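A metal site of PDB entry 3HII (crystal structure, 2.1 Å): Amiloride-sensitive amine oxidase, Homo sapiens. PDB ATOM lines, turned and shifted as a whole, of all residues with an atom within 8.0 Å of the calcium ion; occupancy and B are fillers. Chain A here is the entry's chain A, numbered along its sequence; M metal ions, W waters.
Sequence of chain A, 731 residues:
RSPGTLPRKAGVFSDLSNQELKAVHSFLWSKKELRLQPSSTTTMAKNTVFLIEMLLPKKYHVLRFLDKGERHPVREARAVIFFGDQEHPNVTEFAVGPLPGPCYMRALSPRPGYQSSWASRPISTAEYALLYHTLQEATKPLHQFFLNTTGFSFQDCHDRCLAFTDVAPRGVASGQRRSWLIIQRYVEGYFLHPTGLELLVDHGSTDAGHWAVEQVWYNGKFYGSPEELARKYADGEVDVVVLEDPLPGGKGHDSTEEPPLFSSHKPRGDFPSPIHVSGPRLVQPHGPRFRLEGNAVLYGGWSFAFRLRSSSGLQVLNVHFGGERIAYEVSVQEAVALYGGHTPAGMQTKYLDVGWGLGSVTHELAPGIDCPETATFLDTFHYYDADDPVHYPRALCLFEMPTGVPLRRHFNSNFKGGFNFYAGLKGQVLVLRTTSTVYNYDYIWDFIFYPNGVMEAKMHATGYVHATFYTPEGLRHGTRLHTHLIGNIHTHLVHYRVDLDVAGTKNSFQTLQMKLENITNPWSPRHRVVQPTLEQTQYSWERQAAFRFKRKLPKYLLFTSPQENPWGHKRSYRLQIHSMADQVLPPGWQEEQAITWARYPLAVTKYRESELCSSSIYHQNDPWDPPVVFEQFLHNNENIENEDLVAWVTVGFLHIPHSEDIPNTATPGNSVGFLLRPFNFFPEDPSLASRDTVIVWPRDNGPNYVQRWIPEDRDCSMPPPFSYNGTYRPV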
ATOM      1  N   GLU A 542       5.367  -6.289   7.239  1.00  0.00           N
ATOM      2  CA  GLU A 542       6.009  -5.742   8.441  1.00  0.00           C
ATOM      3  C   GLU A 542       7.409  -6.308   8.666  1.00  0.00           C
ATOM      4  O   GLU A 542       8.336  -5.547   8.920  1.00  0.00           O
ATOM      5  CB  GLU A 542       5.148  -5.993   9.675  1.00  0.00           C
ATOM      6  CG  GLU A 542       3.874  -5.166   9.720  1.00  0.00           C
ATOM      7  CD  GLU A 542       3.009  -5.508  10.906  1.00  0.00           C
ATOM      8  OE1 GLU A 542       2.803  -6.715  11.183  1.00  0.00           O
ATOM      9  OE2 GLU A 542       2.505  -4.560  11.578  1.00  0.00           O
ATOM     10  N   ARG A 543       7.558  -7.625   8.563  1.00  0.00           N
ATOM     11  CA  ARG A 543       8.825  -8.290   8.868  1.00  0.00           C
ATOM     12  C   ARG A 543       9.952  -7.792   7.973  1.00  0.00           C
ATOM     13  O   ARG A 543      11.106  -7.755   8.388  1.00  0.00           O
ATOM     14  CB  ARG A 543       8.704  -9.817   8.740  1.00  0.00           C
ATOM     15  CG  ARG A 543       7.889 -10.508   9.844  1.00  0.00           C
ATOM     16  CD  ARG A 543       8.620 -10.589  11.184  1.00  0.00           C
ATOM     17  NE  ARG A 543       8.004 -11.570  12.086  1.00  0.00           N
ATOM     18  CZ  ARG A 543       8.424 -11.832  13.331  1.00  0.00           C
ATOM     19  NH1 ARG A 543       9.454 -11.197  13.857  1.00  0.00           N
ATOM     20  NH2 ARG A 543       7.793 -12.752  14.049  1.00  0.00           N
ATOM     21  N   VAL A 604       8.500  -1.051  11.508  1.00  0.00           N
ATOM     22  CA  VAL A 604       7.279  -0.407  11.026  1.00  0.00           C
ATOM     23  C   VAL A 604       6.096  -1.331  11.287  1.00  0.00           C
ATOM     24  O   VAL A 604       6.168  -2.512  10.949  1.00  0.00           O
ATOM     25  CB  VAL A 604       7.402  -0.090   9.507  1.00  0.00           C
ATOM     26  CG1 VAL A 604       6.166   0.625   8.990  1.00  0.00           C
ATOM     27  CG2 VAL A 604       8.664   0.742   9.251  1.00  0.00           C
ATOM     28  N   THR A 605       5.042  -0.826  11.912  1.00  0.00           N
ATOM     29  CA  THR A 605       3.836  -1.645  12.126  1.00  0.00           C
ATOM     30  C   THR A 605       2.594  -1.045  11.503  1.00  0.00           C
ATOM     31  O   THR A 605       2.542   0.142  11.194  1.00  0.00           O
ATOM     32  CB  THR A 605       3.564  -1.941  13.630  1.00  0.00           C
ATOM     33  OG1 THR A 605       3.355  -0.721  14.369  1.00  0.00           O
ATOM     34  CG2 THR A 605       4.717  -2.737  14.238  1.00  0.00           C
ATOM     35  N   LYS A 606       1.591  -1.879  11.280  1.00  0.00           N
ATOM     36  CA  LYS A 606       0.273  -1.394  10.906  1.00  0.00           C
ATOM     37  C   LYS A 606      -0.424  -0.842  12.151  1.00  0.00           C
ATOM     38  O   LYS A 606      -0.471  -1.507  13.183  1.00  0.00           O
ATOM     39  CB  LYS A 606      -0.548  -2.522  10.310  1.00  0.00           C
ATOM     40  CG  LYS A 606      -2.016  -2.159  10.059  1.00  0.00           C
ATOM     41  CD  LYS A 606      -2.680  -3.222   9.211  1.00  0.00           C
ATOM     42  CE  LYS A 606      -4.203  -3.044   9.203  1.00  0.00           C
ATOM     43  NZ  LYS A 606      -4.730  -3.673   7.973  1.00  0.00           N
ATOM     44  N   TYR A 607      -0.949   0.375  12.047  1.00  0.00           N
ATOM     45  CA  TYR A 607      -1.646   1.037  13.155  1.00  0.00           C
ATOM     46  C   TYR A 607      -2.756   0.163  13.766  1.00  0.00           C
ATOM     47  O   TYR A 607      -3.468  -0.536  13.057  1.00  0.00           O
ATOM     48  CB  TYR A 607      -2.254   2.367  12.714  1.00  0.00           C
ATOM     49  CG  TYR A 607      -2.915   3.116  13.852  1.00  0.00           C
ATOM     50  CD1 TYR A 607      -4.245   2.883  14.185  1.00  0.00           C
ATOM     51  CD2 TYR A 607      -2.199   4.060  14.612  1.00  0.00           C
ATOM     52  CE1 TYR A 607      -4.845   3.552  15.246  1.00  0.00           C
ATOM     53  CE2 TYR A 607      -2.808   4.741  15.664  1.00  0.00           C
ATOM     54  CZ  TYR A 607      -4.126   4.482  15.981  1.00  0.00           C
ATOM     55  OH  TYR A 607      -4.703   5.147  17.023  1.00  0.00           O
ATOM     56  N   ARG A 608      -2.870   0.236  15.083  1.00  0.00           N
ATOM     57  CA  ARG A 608      -3.884  -0.502  15.810  1.00  0.00           C
ATOM     58  C   ARG A 608      -4.046   0.111  17.200  1.00  0.00           C
ATOM     59  O   ARG A 608      -3.049   0.370  17.877  1.00  0.00           O
ATOM     60  CB  ARG A 608      -3.433  -1.964  15.928  1.00  0.00           C
ATOM     61  CG  ARG A 608      -4.462  -2.887  16.464  1.00  0.00           C
ATOM     62  CD  ARG A 608      -4.108  -4.338  16.194  1.00  0.00           C
ATOM     63  NE  ARG A 608      -4.462  -4.659  14.814  1.00  0.00           N
ATOM     64  CZ  ARG A 608      -3.611  -4.981  13.845  1.00  0.00           C
ATOM     65  NH1 ARG A 608      -2.309  -5.091  14.061  1.00  0.00           N
ATOM     66  NH2 ARG A 608      -4.100  -5.223  12.647  1.00  0.00           N
ATOM     67  N   GLU A 611      -2.322  -1.338  20.053  1.00  0.00           N
ATOM     68  CA  GLU A 611      -0.848  -1.288  19.983  1.00  0.00           C
ATOM     69  C   GLU A 611      -0.292   0.142  20.029  1.00  0.00           C
ATOM     70  O   GLU A 611       0.668   0.479  19.316  1.00  0.00           O
ATOM     71  CB  GLU A 611      -0.338  -1.981  18.702  1.00  0.00           C
ATOM     72  CG  GLU A 611      -0.731  -3.433  18.568  1.00  0.00           C
ATOM     73  CD  GLU A 611      -0.306  -4.055  17.244  1.00  0.00           C
ATOM     74  OE1 GLU A 611       0.470  -3.420  16.485  1.00  0.00           O
ATOM     75  OE2 GLU A 611      -0.765  -5.174  16.954  1.00  0.00           O
ATOM     76  N   PHE A 630       6.738  -5.902  22.394  1.00  0.00           N
ATOM     77  CA  PHE A 630       6.754  -5.253  21.081  1.00  0.00           C
ATOM     78  C   PHE A 630       6.889  -6.258  19.942  1.00  0.00           C
ATOM     79  O   PHE A 630       6.249  -6.099  18.889  1.00  0.00           O
ATOM     80  CB  PHE A 630       7.861  -4.195  21.005  1.00  0.00           C
ATOM     81  CG  PHE A 630       7.963  -3.552  19.649  1.00  0.00           C
ATOM     82  CD1 PHE A 630       7.118  -2.507  19.303  1.00  0.00           C
ATOM     83  CD2 PHE A 630       8.860  -4.035  18.704  1.00  0.00           C
ATOM     84  CE1 PHE A 630       7.195  -1.934  18.050  1.00  0.00           C
ATOM     85  CE2 PHE A 630       8.939  -3.460  17.442  1.00  0.00           C
ATOM     86  CZ  PHE A 630       8.102  -2.408  17.110  1.00  0.00           C
ATOM     87  N   GLU A 631       7.704  -7.294  20.140  1.00  0.00           N
ATOM     88  CA  GLU A 631       7.892  -8.352  19.119  1.00  0.00           C
ATOM     89  C   GLU A 631       6.575  -8.945  18.627  1.00  0.00           C
ATOM     90  O   GLU A 631       6.434  -9.297  17.457  1.00  0.00           O
ATOM     91  CB  GLU A 631       8.799  -9.474  19.672  1.00  0.00           C
ATOM     92  CG  GLU A 631       9.110 -10.626  18.705  1.00  0.00           C
ATOM     93  CD  GLU A 631      10.067 -10.247  17.584  1.00  0.00           C
ATOM     94  OE1 GLU A 631      10.719  -9.184  17.655  1.00  0.00           O
ATOM     95  OE2 GLU A 631      10.168 -11.032  16.619  1.00  0.00           O
ATOM     96  N   GLN A 632       5.581  -9.011  19.517  1.00  0.00           N
ATOM     97  CA  GLN A 632       4.285  -9.560  19.166  1.00  0.00           C
ATOM     98  C   GLN A 632       3.547  -8.741  18.120  1.00  0.00           C
ATOM     99  O   GLN A 632       2.730  -9.287  17.376  1.00  0.00           O
ATOM    100  CB  GLN A 632       3.430  -9.787  20.428  1.00  0.00           C
ATOM    101  CG  GLN A 632       4.000 -10.853  21.370  1.00  0.00           C
ATOM    102  CD  GLN A 632       3.183 -11.084  22.647  1.00  0.00           C
ATOM    103  OE1 GLN A 632       2.172 -10.409  22.896  1.00  0.00           O
ATOM    104  NE2 GLN A 632       3.619 -12.036  23.466  1.00  0.00           N
ATOM    105  N   PHE A 633       3.849  -7.437  18.031  1.00  0.00           N
ATOM    106  CA  PHE A 633       3.261  -6.575  16.997  1.00  0.00           C
ATOM    107  C   PHE A 633       3.718  -7.008  15.595  1.00  0.00           C
ATOM    108  O   PHE A 633       3.052  -6.707  14.590  1.00  0.00           O
ATOM    109  CB  PHE A 633       3.665  -5.099  17.193  1.00  0.00           C
ATOM    110  CG  PHE A 633       3.260  -4.477  18.520  1.00  0.00           C
ATOM    111  CD1 PHE A 633       2.460  -5.139  19.446  1.00  0.00           C
ATOM    112  CD2 PHE A 633       3.661  -3.181  18.800  1.00  0.00           C
ATOM    113  CE1 PHE A 633       2.104  -4.530  20.640  1.00  0.00           C
ATOM    114  CE2 PHE A 633       3.296  -2.560  19.986  1.00  0.00           C
ATOM    115  CZ  PHE A 633       2.517  -3.240  20.909  1.00  0.00           C
ATOM    116  N   LEU A 634       4.865  -7.686  15.522  1.00  0.00           N
ATOM    117  CA  LEU A 634       5.435  -8.161  14.250  1.00  0.00           C
ATOM    118  C   LEU A 634       4.993  -9.584  13.896  1.00  0.00           C
ATOM    119  O   LEU A 634       5.142 -10.005  12.748  1.00  0.00           O
ATOM    120  CB  LEU A 634       6.971  -8.106  14.315  1.00  0.00           C
ATOM    121  CG  LEU A 634       7.615  -6.780  14.743  1.00  0.00           C
ATOM    122  CD1 LEU A 634       9.125  -6.963  14.915  1.00  0.00           C
ATOM    123  CD2 LEU A 634       7.329  -5.683  13.724  1.00  0.00           C
ATOM    124  N   HIS A 635       4.471 -10.329  14.858  1.00  0.00           N
ATOM    125  CA  HIS A 635       4.101 -11.725  14.638  1.00  0.00           C
ATOM    126  C   HIS A 635       3.186 -11.974  13.451  1.00  0.00           C
ATOM    127  O   HIS A 635       3.410 -12.904  12.682  1.00  0.00           O
ATOM    128  CB  HIS A 635       3.467 -12.329  15.898  1.00  0.00           C
ATOM    129  CG  HIS A 635       4.446 -12.658  16.971  1.00  0.00           C
ATOM    130  ND1 HIS A 635       4.066 -13.066  18.228  1.00  0.00           N
ATOM    131  CD2 HIS A 635       5.799 -12.623  16.973  1.00  0.00           C
ATOM    132  CE1 HIS A 635       5.154 -13.295  18.957  1.00  0.00           C
ATOM    133  NE2 HIS A 635       6.218 -13.030  18.218  1.00  0.00           N
ATOM    134  N   ASN A 636       2.140 -11.168  13.302  1.00  0.00           N
ATOM    135  CA  ASN A 636       1.201 -11.361  12.212  1.00  0.00           C
ATOM    136  C   ASN A 636       1.688 -10.836  10.846  1.00  0.00           C
ATOM    137  O   ASN A 636       1.011 -11.014   9.838  1.00  0.00           O
ATOM    138  CB  ASN A 636      -0.191 -10.838  12.584  1.00  0.00           C
ATOM    139  CG  ASN A 636      -0.209  -9.370  12.979  1.00  0.00           C
ATOM    140  OD1 ASN A 636       0.795  -8.660  12.831  1.00  0.00           O
ATOM    141  ND2 ASN A 636      -1.341  -8.913  13.506  1.00  0.00           N
ATOM    142  N   ASN A 637       2.856 -10.198  10.826  1.00  0.00           N
ATOM    143  CA  ASN A 637       3.537  -9.835   9.577  1.00  0.00           C
ATOM    144  C   ASN A 637       2.607  -9.239   8.525  1.00  0.00           C
ATOM    145  O   ASN A 637       2.532  -9.723   7.389  1.00  0.00           O
ATOM    146  CB  ASN A 637       4.271 -11.035   8.982  1.00  0.00           C
ATOM    147  CG  ASN A 637       5.235 -10.621   7.883  1.00  0.00           C
ATOM    148  OD1 ASN A 637       5.644  -9.466   7.819  1.00  0.00           O
ATOM    149  ND2 ASN A 637       5.586 -11.557   7.004  1.00  0.00           N
ATOM    150  N   GLU A 638       1.933  -8.163   8.904  1.00  0.00           N
ATOM    151  CA  GLU A 638       0.859  -7.628   8.086  1.00  0.00           C
ATOM    152  C   GLU A 638       1.345  -6.868   6.882  1.00  0.00           C
ATOM    153  O   GLU A 638       2.482  -6.363   6.851  1.00  0.00           O
ATOM    154  CB  GLU A 638      -0.032  -6.731   8.930  1.00  0.00           C
ATOM    155  CG  GLU A 638      -0.672  -7.460  10.079  1.00  0.00           C
ATOM    156  CD  GLU A 638      -1.442  -6.540  10.999  1.00  0.00           C
ATOM    157  OE1 GLU A 638      -0.823  -5.979  11.929  1.00  0.00           O
ATOM    158  OE2 GLU A 638      -2.665  -6.399  10.793  1.00  0.00           O
ATOM    159  N   ASN A 639       0.487  -6.812   5.874  1.00  0.00           N
ATOM    160  CA  ASN A 639       0.779  -6.071   4.678  1.00  0.00           C
ATOM    161  C   ASN A 639       0.857  -4.600   5.036  1.00  0.00           C
ATOM    162  O   ASN A 639       0.018  -4.110   5.781  1.00  0.00           O
ATOM    163  CB  ASN A 639      -0.293  -6.304   3.599  1.00  0.00           C
ATOM    164  CG  ASN A 639       0.112  -5.743   2.242  1.00  0.00           C
ATOM    165  OD1 ASN A 639       0.019  -4.540   2.016  1.00  0.00           O
ATOM    166  ND2 ASN A 639       0.567  -6.618   1.343  1.00  0.00           N
ATOM    167  N   ILE A 640       1.882  -3.922   4.524  1.00  0.00           N
ATOM    168  CA  ILE A 640       2.079  -2.502   4.821  1.00  0.00           C
ATOM    169  C   ILE A 640       2.138  -1.619   3.570  1.00  0.00           C
ATOM    170  O   ILE A 640       2.747  -0.542   3.586  1.00  0.00           O
ATOM    171  CB  ILE A 640       3.319  -2.283   5.710  1.00  0.00           C
ATOM    172  CG1 ILE A 640       4.568  -2.890   5.063  1.00  0.00           C
ATOM    173  CG2 ILE A 640       3.047  -2.855   7.124  1.00  0.00           C
ATOM    174  CD1 ILE A 640       5.872  -2.467   5.715  1.00  0.00           C
HETATM  175 CA    CA M   1       1.301  -6.272  13.123  1.00  0.00          CA
HETATM  176  O   HOH W   1       0.091  -6.808  15.034  1.00  0.00           O
HETATM  177  O   HOH W   2       0.657  -4.143  13.975  1.00  0.00           O
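Arg 608 touches the calcium ion.
Along chain A the residues within 4 Å of the calcium ion span positions 542 to 638.
The side-chain carboxylate (OE2) of Glu 542 lies close to the backbone NH (N) of Lys 606, at 2.8 Å.
NH2 of Arg 608 lies within salt-bridge range of OE2 of Glu 638, at 2.6 Å.
The side-chain carboxylate (OE2) of Glu 611 lies within salt-bridge range of the guanidinium group (NH1) of Arg 608, 3.3 Å away.
OD1 of Asn 637 is in hydrogen-bond range of N of Glu 542, at 3.2 Å.
The calcium ion is bound by water W1 (2.3 Å), O of Phe 633 (2.3 Å), water W2 (2.4 Å), OE1 of Glu 638 (2.5 Å), OD1 of Asn 636 (2.5 Å), OE1 of Glu 542 (2.5 Å) and OE2 of Glu 542 (2.6 Å).
Water W1 lies within hydrogen-bond range of the side-chain carboxylate of Glu 611 (2.7 Å), the side-chain amide nitrogen of Asn 636 (3.0 Å) and the guanidinium group of Arg 608 (3.1 Å).
Water W2 lies within hydrogen-bond range of OE1 of Glu 611 (2.6 Å), O of Lys 606 (3.0 Å) and NH1 of Arg 608 (3.1 Å).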
